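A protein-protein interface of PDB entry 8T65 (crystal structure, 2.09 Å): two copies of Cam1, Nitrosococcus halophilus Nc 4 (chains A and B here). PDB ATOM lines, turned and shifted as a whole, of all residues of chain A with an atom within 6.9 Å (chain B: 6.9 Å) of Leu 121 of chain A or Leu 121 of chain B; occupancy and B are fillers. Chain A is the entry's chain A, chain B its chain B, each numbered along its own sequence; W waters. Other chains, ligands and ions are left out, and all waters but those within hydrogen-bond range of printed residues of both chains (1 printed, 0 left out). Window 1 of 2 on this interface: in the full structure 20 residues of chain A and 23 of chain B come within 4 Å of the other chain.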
ATOM      1  N   PRO A  87      25.396  29.918  19.500  1.00  0.00           N
ATOM      2  CA  PRO A  87      24.688  28.662  19.219  1.00  0.00           C
ATOM      3  C   PRO A  87      24.285  28.500  17.762  1.00  0.00           C
ATOM      4  O   PRO A  87      23.828  27.410  17.377  1.00  0.00           O
ATOM      5  CB  PRO A  87      23.463  28.733  20.136  1.00  0.00           C
ATOM      6  CG  PRO A  87      23.254  30.196  20.378  1.00  0.00           C
ATOM      7  CD  PRO A  87      24.594  30.855  20.309  1.00  0.00           C
ATOM      8  N   PRO A  90      27.737  26.039  13.794  1.00  0.00           N
ATOM      9  CA  PRO A  90      28.072  24.620  14.001  1.00  0.00           C
ATOM     10  C   PRO A  90      29.550  24.391  14.241  1.00  0.00           C
ATOM     11  O   PRO A  90      29.910  23.425  14.920  1.00  0.00           O
ATOM     12  CB  PRO A  90      27.587  23.950  12.707  1.00  0.00           C
ATOM     13  CG  PRO A  90      27.528  25.055  11.701  1.00  0.00           C
ATOM     14  CD  PRO A  90      27.214  26.307  12.441  1.00  0.00           C
ATOM     15  N   LEU A 116      22.548  14.254  20.529  1.00  0.00           N
ATOM     16  CA  LEU A 116      22.473  15.562  19.902  1.00  0.00           C
ATOM     17  C   LEU A 116      21.052  16.120  19.876  1.00  0.00           C
ATOM     18  O   LEU A 116      20.784  17.057  19.116  1.00  0.00           O
ATOM     19  CB  LEU A 116      23.072  15.500  18.498  1.00  0.00           C
ATOM     20  CG  LEU A 116      22.788  14.275  17.637  1.00  0.00           C
ATOM     21  CD1 LEU A 116      21.312  14.167  17.277  1.00  0.00           C
ATOM     22  CD2 LEU A 116      23.654  14.352  16.375  1.00  0.00           C
ATOM     23  N   THR A 117      20.147  15.573  20.699  1.00  0.00           N
ATOM     24  CA  THR A 117      18.764  16.051  20.710  1.00  0.00           C
ATOM     25  C   THR A 117      18.696  17.529  21.090  1.00  0.00           C
ATOM     26  O   THR A 117      18.064  18.330  20.393  1.00  0.00           O
ATOM     27  CB  THR A 117      17.898  15.216  21.665  1.00  0.00           C
ATOM     28  OG1 THR A 117      18.084  13.821  21.399  1.00  0.00           O
ATOM     29  CG2 THR A 117      16.401  15.560  21.485  1.00  0.00           C
ATOM     30  N   GLY A 118      19.365  17.918  22.184  1.00  0.00           N
ATOM     31  CA  GLY A 118      19.223  19.262  22.713  1.00  0.00           C
ATOM     32  C   GLY A 118      20.007  20.320  21.944  1.00  0.00           C
ATOM     33  O   GLY A 118      20.769  20.041  21.023  1.00  0.00           O
ATOM     34  N   GLY A 119      19.798  21.573  22.339  1.00  0.00           N
ATOM     35  CA  GLY A 119      20.433  22.700  21.683  1.00  0.00           C
ATOM     36  C   GLY A 119      19.742  23.101  20.389  1.00  0.00           C
ATOM     37  O   GLY A 119      18.839  22.431  19.886  1.00  0.00           O
ATOM     38  N   LYS A 120      20.187  24.234  19.843  1.00  0.00           N
ATOM     39  CA  LYS A 120      19.752  24.668  18.528  1.00  0.00           C
ATOM     40  C   LYS A 120      20.272  23.696  17.467  1.00  0.00           C
ATOM     41  O   LYS A 120      21.233  22.957  17.689  1.00  0.00           O
ATOM     42  CB  LYS A 120      20.261  26.084  18.244  1.00  0.00           C
ATOM     43  CG  LYS A 120      19.894  27.133  19.326  1.00  0.00           C
ATOM     44  CD  LYS A 120      20.199  28.555  18.843  1.00  0.00           C
ATOM     45  CE  LYS A 120      19.011  29.188  18.115  1.00  0.00           C
ATOM     46  NZ  LYS A 120      19.291  30.607  17.697  1.00  0.00           N
ATOM     47  N   LEU A 121      19.626  23.708  16.303  1.00  0.00           N
ATOM     48  CA  LEU A 121      20.030  22.818  15.215  1.00  0.00           C
ATOM     49  C   LEU A 121      21.512  22.922  14.851  1.00  0.00           C
ATOM     50  O   LEU A 121      22.140  21.866  14.668  1.00  0.00           O
ATOM     51  CB  LEU A 121      19.130  23.077  13.993  1.00  0.00           C
ATOM     52  CG  LEU A 121      19.333  22.316  12.683  1.00  0.00           C
ATOM     53  CD1 LEU A 121      19.420  20.850  12.928  1.00  0.00           C
ATOM     54  CD2 LEU A 121      18.177  22.578  11.730  1.00  0.00           C
ATOM     55  N   PRO A 122      22.128  24.106  14.718  1.00  0.00           N
ATOM     56  CA  PRO A 122      23.574  24.136  14.423  1.00  0.00           C
ATOM     57  C   PRO A 122      24.434  23.522  15.514  1.00  0.00           C
ATOM     58  O   PRO A 122      25.522  23.023  15.209  1.00  0.00           O
ATOM     59  CB  PRO A 122      23.880  25.637  14.255  1.00  0.00           C
ATOM     60  CG  PRO A 122      22.582  26.250  13.890  1.00  0.00           C
ATOM     61  CD  PRO A 122      21.536  25.455  14.641  1.00  0.00           C
ATOM     62  N   MET A 123      23.995  23.571  16.777  1.00  0.00           N
ATOM     63  CA  MET A 123      24.693  22.848  17.839  1.00  0.00           C
ATOM     64  C   MET A 123      24.650  21.344  17.596  1.00  0.00           C
ATOM     65  O   MET A 123      25.671  20.654  17.730  1.00  0.00           O
ATOM     66  CB  MET A 123      24.081  23.185  19.204  1.00  0.00           C
ATOM     67  CG  MET A 123      24.239  24.648  19.618  1.00  0.00           C
ATOM     68  SD  MET A 123      23.333  25.093  21.128  1.00  0.00           S
ATOM     69  CE  MET A 123      24.375  24.317  22.374  1.00  0.00           C
ATOM     70  N   SER A 124      23.465  20.816  17.251  1.00  0.00           N
ATOM     71  CA  SER A 124      23.343  19.389  16.973  1.00  0.00           C
ATOM     72  C   SER A 124      24.190  19.002  15.776  1.00  0.00           C
ATOM     73  O   SER A 124      24.799  17.923  15.746  1.00  0.00           O
ATOM     74  CB  SER A 124      21.879  19.031  16.722  1.00  0.00           C
ATOM     75  OG  SER A 124      21.118  19.259  17.903  1.00  0.00           O
ATOM     76  N   LEU A 125      24.263  19.888  14.789  1.00  0.00           N
ATOM     77  CA  LEU A 125      25.021  19.580  13.584  1.00  0.00           C
ATOM     78  C   LEU A 125      26.516  19.608  13.855  1.00  0.00           C
ATOM     79  O   LEU A 125      27.252  18.747  13.361  1.00  0.00           O
ATOM     80  CB  LEU A 125      24.656  20.560  12.471  1.00  0.00           C
ATOM     81  CG  LEU A 125      25.403  20.275  11.176  1.00  0.00           C
ATOM     82  CD1 LEU A 125      24.907  18.967  10.558  1.00  0.00           C
ATOM     83  CD2 LEU A 125      25.249  21.432  10.211  1.00  0.00           C
ATOM     84  N   GLY A 126      26.988  20.591  14.627  1.00  0.00           N
ATOM     85  CA  GLY A 126      28.378  20.566  15.054  1.00  0.00           C
ATOM     86  C   GLY A 126      28.711  19.312  15.841  1.00  0.00           C
ATOM     87  O   GLY A 126      29.712  18.638  15.574  1.00  0.00           O
ATOM     88  N   ALA A 127      27.851  18.965  16.800  1.00  0.00           N
ATOM     89  CA  ALA A 127      28.046  17.750  17.592  1.00  0.00           C
ATOM     90  C   ALA A 127      28.108  16.518  16.708  1.00  0.00           C
ATOM     91  O   ALA A 127      28.954  15.648  16.914  1.00  0.00           O
ATOM     92  CB  ALA A 127      26.917  17.602  18.615  1.00  0.00           C
ATOM     93  N   LEU A 139      23.179   9.757  19.150  1.00  0.00           N
ATOM     94  CA  LEU A 139      21.870   9.331  19.624  1.00  0.00           C
ATOM     95  C   LEU A 139      20.841  10.437  19.441  1.00  0.00           C
ATOM     96  O   LEU A 139      21.183  11.621  19.377  1.00  0.00           O
ATOM     97  CB  LEU A 139      21.920   8.939  21.103  1.00  0.00           C
ATOM     98  CG  LEU A 139      23.129   8.104  21.510  1.00  0.00           C
ATOM     99  CD1 LEU A 139      23.050   7.779  23.006  1.00  0.00           C
ATOM    100  CD2 LEU A 139      23.191   6.843  20.664  1.00  0.00           C
ATOM    101  N   TYR A 140      19.567  10.031  19.406  1.00  0.00           N
ATOM    102  CA  TYR A 140      18.450  10.952  19.214  1.00  0.00           C
ATOM    103  C   TYR A 140      17.234  10.450  19.990  1.00  0.00           C
ATOM    104  O   TYR A 140      16.876   9.270  19.887  1.00  0.00           O
ATOM    105  CB  TYR A 140      18.110  11.090  17.726  1.00  0.00           C
ATOM    106  CG  TYR A 140      16.890  11.941  17.432  1.00  0.00           C
ATOM    107  CD1 TYR A 140      16.880  13.297  17.714  1.00  0.00           C
ATOM    108  CD2 TYR A 140      15.753  11.381  16.881  1.00  0.00           C
ATOM    109  CE1 TYR A 140      15.768  14.074  17.459  1.00  0.00           C
ATOM    110  CE2 TYR A 140      14.637  12.142  16.606  1.00  0.00           C
ATOM    111  CZ  TYR A 140      14.646  13.493  16.893  1.00  0.00           C
ATOM    112  OH  TYR A 140      13.529  14.252  16.622  1.00  0.00           O
ATOM    113  N   ILE A 162      21.350   7.041  15.627  1.00  0.00           N
ATOM    114  CA  ILE A 162      21.245   7.465  14.237  1.00  0.00           C
ATOM    115  C   ILE A 162      22.551   7.327  13.483  1.00  0.00           C
ATOM    116  O   ILE A 162      22.570   7.564  12.270  1.00  0.00           O
ATOM    117  CB  ILE A 162      20.701   8.897  14.114  1.00  0.00           C
ATOM    118  CG1 ILE A 162      21.610   9.895  14.806  1.00  0.00           C
ATOM    119  CG2 ILE A 162      19.298   8.985  14.683  1.00  0.00           C
ATOM    120  CD1 ILE A 162      20.963  11.252  14.901  1.00  0.00           C
ATOM    121  N   PRO B  87      10.266   9.802   9.506  1.00  0.00           N
ATOM    122  CA  PRO B  87      10.986  11.048   9.798  1.00  0.00           C
ATOM    123  C   PRO B  87      12.076  10.905  10.851  1.00  0.00           C
ATOM    124  O   PRO B  87      12.849  11.853  11.025  1.00  0.00           O
ATOM    125  CB  PRO B  87       9.875  11.989  10.287  1.00  0.00           C
ATOM    126  CG  PRO B  87       8.868  11.084  10.860  1.00  0.00           C
ATOM    127  CD  PRO B  87       8.871   9.863   9.965  1.00  0.00           C
ATOM    128  N   PRO B  90      17.496   9.430   9.207  1.00  0.00           N
ATOM    129  CA  PRO B  90      18.120  10.379   8.263  1.00  0.00           C
ATOM    130  C   PRO B  90      18.198   9.882   6.826  1.00  0.00           C
ATOM    131  O   PRO B  90      18.151  10.704   5.902  1.00  0.00           O
ATOM    132  CB  PRO B  90      19.527  10.595   8.849  1.00  0.00           C
ATOM    133  CG  PRO B  90      19.448  10.153  10.268  1.00  0.00           C
ATOM    134  CD  PRO B  90      18.386   9.084  10.330  1.00  0.00           C
ATOM    135  N   LEU B 116      17.447  23.484   5.756  1.00  0.00           N
ATOM    136  CA  LEU B 116      17.142  22.336   6.591  1.00  0.00           C
ATOM    137  C   LEU B 116      16.520  22.732   7.923  1.00  0.00           C
ATOM    138  O   LEU B 116      16.484  21.914   8.846  1.00  0.00           O
ATOM    139  CB  LEU B 116      18.401  21.500   6.801  1.00  0.00           C
ATOM    140  CG  LEU B 116      19.697  22.256   7.037  1.00  0.00           C
ATOM    141  CD1 LEU B 116      19.710  22.874   8.425  1.00  0.00           C
ATOM    142  CD2 LEU B 116      20.871  21.302   6.850  1.00  0.00           C
ATOM    143  N   THR B 117      16.017  23.964   8.034  1.00  0.00           N
ATOM    144  CA  THR B 117      15.445  24.420   9.298  1.00  0.00           C
ATOM    145  C   THR B 117      14.289  23.530   9.744  1.00  0.00           C
ATOM    146  O   THR B 117      14.182  23.192  10.930  1.00  0.00           O
ATOM    147  CB  THR B 117      14.972  25.874   9.178  1.00  0.00           C
ATOM    148  OG1 THR B 117      15.995  26.684   8.573  1.00  0.00           O
ATOM    149  CG2 THR B 117      14.618  26.440  10.557  1.00  0.00           C
ATOM    150  N   GLY B 118      13.403  23.149   8.813  1.00  0.00           N
ATOM    151  CA  GLY B 118      12.185  22.453   9.177  1.00  0.00           C
ATOM    152  C   GLY B 118      12.367  20.950   9.296  1.00  0.00           C
ATOM    153  O   GLY B 118      13.399  20.390   8.948  1.00  0.00           O
ATOM    154  N   GLY B 119      11.326  20.291   9.793  1.00  0.00           N
ATOM    155  CA  GLY B 119      11.366  18.859  10.011  1.00  0.00           C
ATOM    156  C   GLY B 119      11.969  18.493  11.359  1.00  0.00           C
ATOM    157  O   GLY B 119      12.507  19.325  12.092  1.00  0.00           O
ATOM    158  N   LYS B 120      11.864  17.204  11.688  1.00  0.00           N
ATOM    159  CA  LYS B 120      12.588  16.638  12.815  1.00  0.00           C
ATOM    160  C   LYS B 120      14.087  16.721  12.572  1.00  0.00           C
ATOM    161  O   LYS B 120      14.546  16.863  11.442  1.00  0.00           O
ATOM    162  CB  LYS B 120      12.189  15.172  13.043  1.00  0.00           C
ATOM    163  CG  LYS B 120      10.687  14.941  13.194  1.00  0.00           C
ATOM    164  CD  LYS B 120      10.374  13.499  13.607  1.00  0.00           C
ATOM    165  CE  LYS B 120      10.096  13.380  15.093  1.00  0.00           C
ATOM    166  NZ  LYS B 120       9.493  12.042  15.468  1.00  0.00           N
ATOM    167  N   LEU B 121      14.857  16.628  13.661  1.00  0.00           N
ATOM    168  CA  LEU B 121      16.315  16.651  13.551  1.00  0.00           C
ATOM    169  C   LEU B 121      16.859  15.643  12.544  1.00  0.00           C
ATOM    170  O   LEU B 121      17.697  16.034  11.714  1.00  0.00           O
ATOM    171  CB  LEU B 121      16.922  16.435  14.943  1.00  0.00           C
ATOM    172  CG  LEU B 121      18.409  16.679  15.121  1.00  0.00           C
ATOM    173  CD1 LEU B 121      18.754  17.988  14.496  1.00  0.00           C
ATOM    174  CD2 LEU B 121      18.741  16.734  16.601  1.00  0.00           C
ATOM    175  N   PRO B 122      16.444  14.369  12.539  1.00  0.00           N
ATOM    176  CA  PRO B 122      16.975  13.437  11.527  1.00  0.00           C
ATOM    177  C   PRO B 122      16.591  13.796  10.102  1.00  0.00           C
ATOM    178  O   PRO B 122      17.299  13.401   9.173  1.00  0.00           O
ATOM    179  CB  PRO B 122      16.370  12.084  11.930  1.00  0.00           C
ATOM    180  CG  PRO B 122      15.885  12.253  13.328  1.00  0.00           C
ATOM    181  CD  PRO B 122      15.495  13.689  13.445  1.00  0.00           C
ATOM    182  N   MET B 123      15.488  14.515   9.892  1.00  0.00           N
ATOM    183  CA  MET B 123      15.166  14.973   8.544  1.00  0.00           C
ATOM    184  C   MET B 123      16.150  16.048   8.099  1.00  0.00           C
ATOM    185  O   MET B 123      16.650  16.014   6.970  1.00  0.00           O
ATOM    186  CB  MET B 123      13.735  15.503   8.502  1.00  0.00           C
ATOM    187  CG  MET B 123      12.658  14.443   8.685  1.00  0.00           C
ATOM    188  SD  MET B 123      11.009  15.183   8.892  1.00  0.00           S
ATOM    189  CE  MET B 123      10.742  15.890   7.267  1.00  0.00           C
ATOM    190  N   SER B 124      16.453  16.993   8.995  1.00  0.00           N
ATOM    191  CA  SER B 124      17.509  17.978   8.759  1.00  0.00           C
ATOM    192  C   SER B 124      18.860  17.323   8.513  1.00  0.00           C
ATOM    193  O   SER B 124      19.644  17.790   7.675  1.00  0.00           O
ATOM    194  CB  SER B 124      17.611  18.928   9.964  1.00  0.00           C
ATOM    195  OG  SER B 124      16.422  19.684  10.124  1.00  0.00           O
ATOM    196  N   LEU B 125      19.183  16.292   9.289  1.00  0.00           N
ATOM    197  CA  LEU B 125      20.502  15.677   9.176  1.00  0.00           C
ATOM    198  C   LEU B 125      20.651  14.933   7.852  1.00  0.00           C
ATOM    199  O   LEU B 125      21.711  14.985   7.222  1.00  0.00           O
ATOM    200  CB  LEU B 125      20.754  14.731  10.353  1.00  0.00           C
ATOM    201  CG  LEU B 125      21.508  15.315  11.554  1.00  0.00           C
ATOM    202  CD1 LEU B 125      20.999  16.699  11.899  1.00  0.00           C
ATOM    203  CD2 LEU B 125      21.425  14.397  12.771  1.00  0.00           C
ATOM    204  N   GLY B 126      19.604  14.227   7.421  1.00  0.00           N
ATOM    205  CA  GLY B 126      19.647  13.583   6.116  1.00  0.00           C
ATOM    206  C   GLY B 126      19.659  14.591   4.985  1.00  0.00           C
ATOM    207  O   GLY B 126      20.344  14.396   3.977  1.00  0.00           O
ATOM    208  N   ALA B 127      18.898  15.684   5.137  1.00  0.00           N
ATOM    209  CA  ALA B 127      18.977  16.803   4.198  1.00  0.00           C
ATOM    210  C   ALA B 127      20.405  17.323   4.065  1.00  0.00           C
ATOM    211  O   ALA B 127      20.901  17.562   2.954  1.00  0.00           O
ATOM    212  CB  ALA B 127      18.050  17.932   4.656  1.00  0.00           C
ATOM    213  N   LEU B 139      21.286  25.947   4.432  1.00  0.00           N
ATOM    214  CA  LEU B 139      20.831  27.171   5.084  1.00  0.00           C
ATOM    215  C   LEU B 139      20.059  26.854   6.356  1.00  0.00           C
ATOM    216  O   LEU B 139      19.519  25.757   6.525  1.00  0.00           O
ATOM    217  CB  LEU B 139      19.925  28.009   4.160  1.00  0.00           C
ATOM    218  CG  LEU B 139      20.365  28.151   2.705  1.00  0.00           C
ATOM    219  CD1 LEU B 139      19.293  28.855   1.872  1.00  0.00           C
ATOM    220  CD2 LEU B 139      21.690  28.911   2.650  1.00  0.00           C
ATOM    221  N   TYR B 140      19.979  27.854   7.233  1.00  0.00           N
ATOM    222  CA  TYR B 140      19.287  27.720   8.504  1.00  0.00           C
ATOM    223  C   TYR B 140      18.700  29.080   8.853  1.00  0.00           C
ATOM    224  O   TYR B 140      19.374  30.105   8.708  1.00  0.00           O
ATOM    225  CB  TYR B 140      20.254  27.242   9.606  1.00  0.00           C
ATOM    226  CG  TYR B 140      19.721  27.307  11.041  1.00  0.00           C
ATOM    227  CD1 TYR B 140      18.702  26.458  11.456  1.00  0.00           C
ATOM    228  CD2 TYR B 140      20.257  28.189  11.977  1.00  0.00           C
ATOM    229  CE1 TYR B 140      18.210  26.498  12.744  1.00  0.00           C
ATOM    230  CE2 TYR B 140      19.783  28.227  13.286  1.00  0.00           C
ATOM    231  CZ  TYR B 140      18.762  27.369  13.660  1.00  0.00           C
ATOM    232  OH  TYR B 140      18.252  27.388  14.952  1.00  0.00           O
ATOM    233  N   ILE B 162      24.846  27.643   6.491  1.00  0.00           N
ATOM    234  CA  ILE B 162      25.489  26.644   7.345  1.00  0.00           C
ATOM    235  C   ILE B 162      26.786  26.127   6.722  1.00  0.00           C
ATOM    236  O   ILE B 162      27.743  25.810   7.440  1.00  0.00           O
ATOM    237  CB  ILE B 162      24.508  25.485   7.623  1.00  0.00           C
ATOM    238  CG1 ILE B 162      23.421  25.914   8.601  1.00  0.00           C
ATOM    239  CG2 ILE B 162      25.226  24.250   8.103  1.00  0.00           C
ATOM    240  CD1 ILE B 162      23.937  26.634   9.826  1.00  0.00           C
HETATM  241  O   HOH W   1      17.078  29.576  15.660  1.00  0.00           O
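OG of Ser 124 of chain A sits at hydrogen-bond distance from O of Leu 116 of chain A, at 2.5 Å. The backbone NH (N) of Leu 116 of chain A lies within hydrogen-bond range of the backbone carbonyl oxygen (O) of Leu 139 of chain A (3.2 Å). The backbone carbonyl oxygen (O) of Gly 118 of chain A sits at hydrogen-bond distance from the side-chain hydroxyl (OG) of Ser 124 of chain A, at 3.2 Å. SD of Met 123 of chain A is in hydrogen-bond range of N of Lys 120 of chain A. O of Gly 118 of chain B is in hydrogen-bond range of OG of Ser 124 of chain B (3.3 Å). The backbone NH (N) of Lys 120 of chain B is in hydrogen-bond range of the side-chain sulfur (SD) of Met 123 of chain B (3.6 Å).
Among the printed residues, pairs that only touch across the chains: Leu 116 of chain A with Leu 121 of chain B, Leu 121 of chain A with Leu 121 of chain B, Leu 121 of chain A with Leu 116 of chain B, Pro 122 of chain A with Tyr 140 of chain B, Tyr 140 of chain A with Pro 122 of chain B, Leu 125 of chain A with Ile 162 of chain B, Tyr 140 of chain A with Leu 121 of chain B, Ser 124 of chain A with Leu 121 of chain B, Lys 120 of chain A with Tyr 140 of chain B, Leu 121 of chain A with Ser 124 of chain B, Leu 121 of chain A with Tyr 140 of chain B, Ile 162 of chain A with Leu 125 of chain B and Tyr 140 of chain A with Lys 120 of chain B.
Of chain B, only Leu 116, Leu 121, Ser 124 and Tyr 140 come within 4 Å of Leu 121 of chain A. Of chain A, only Leu 116 (3.3 Å), Leu 121 (3.3 Å), Ser 124 (3.7 Å) and Tyr 140 (3.6 Å) come within 4 Å of Leu 121 of chain B. Of the printed residues of chain A, Ser 124 of chain B touches Leu 121 (3.7 Å). Of the printed residues of chain B, Ile 162 of chain A touches Leu 125. Printed residues of chain A within 4 Å of Tyr 140 of chain B: Lys 120 (3.7 Å), Leu 121 (3.8 Å) and Pro 122 (3.5 Å). Of the printed residues of chain A, Leu 116 of chain B touches Leu 121 (3.4 Å). Pro 90 of chain B touches none of the printed residues of chain A. Thr 117 of chain B touches none of the printed residues of chain A. The nearest printed residue of chain A that does not touch Tyr 140 of chain B is Pro 87 of chain A (5.8 Å).
Of the 17 printed residues of chain A, 8 touch a printed residue of chain B. Printed residues of chain A that touch a printed residue of chain B: Leu 116, Lys 120, Leu 121, Pro 122, Ser 124, Leu 125, Tyr 140 and Ile 162. Printed residues of chain B that touch a printed residue of chain A: Leu 116, Lys 120, Leu 121, Pro 122, Ser 124, Leu 125, Tyr 140 and Ile 162. Among the printed residues, 13 pairs touch across the chains.
Leu 116 of chain A touches Leu 121 of chain B, and with the chains exchanged Leu 121 of chain A touches Leu 116 of chain B. Lys 120 of chain A touches Tyr 140 of chain B, and with the chains exchanged Tyr 140 of chain A touches Lys 120 of chain B. Leu 121 of chain A touches Ser 124 of chain B, and with the chains exchanged Ser 124 of chain A touches Leu 121 of chain B. Leu 125 of chain A touches Ile 162 of chain B, and with the chains exchanged Ile 162 of chain A touches Leu 125 of chain B.
Water W1 lies within hydrogen-bond range of OH of Tyr 140 of chain B (2.6 Å) and NZ of Lys 120 of chain A (3.2 Å).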
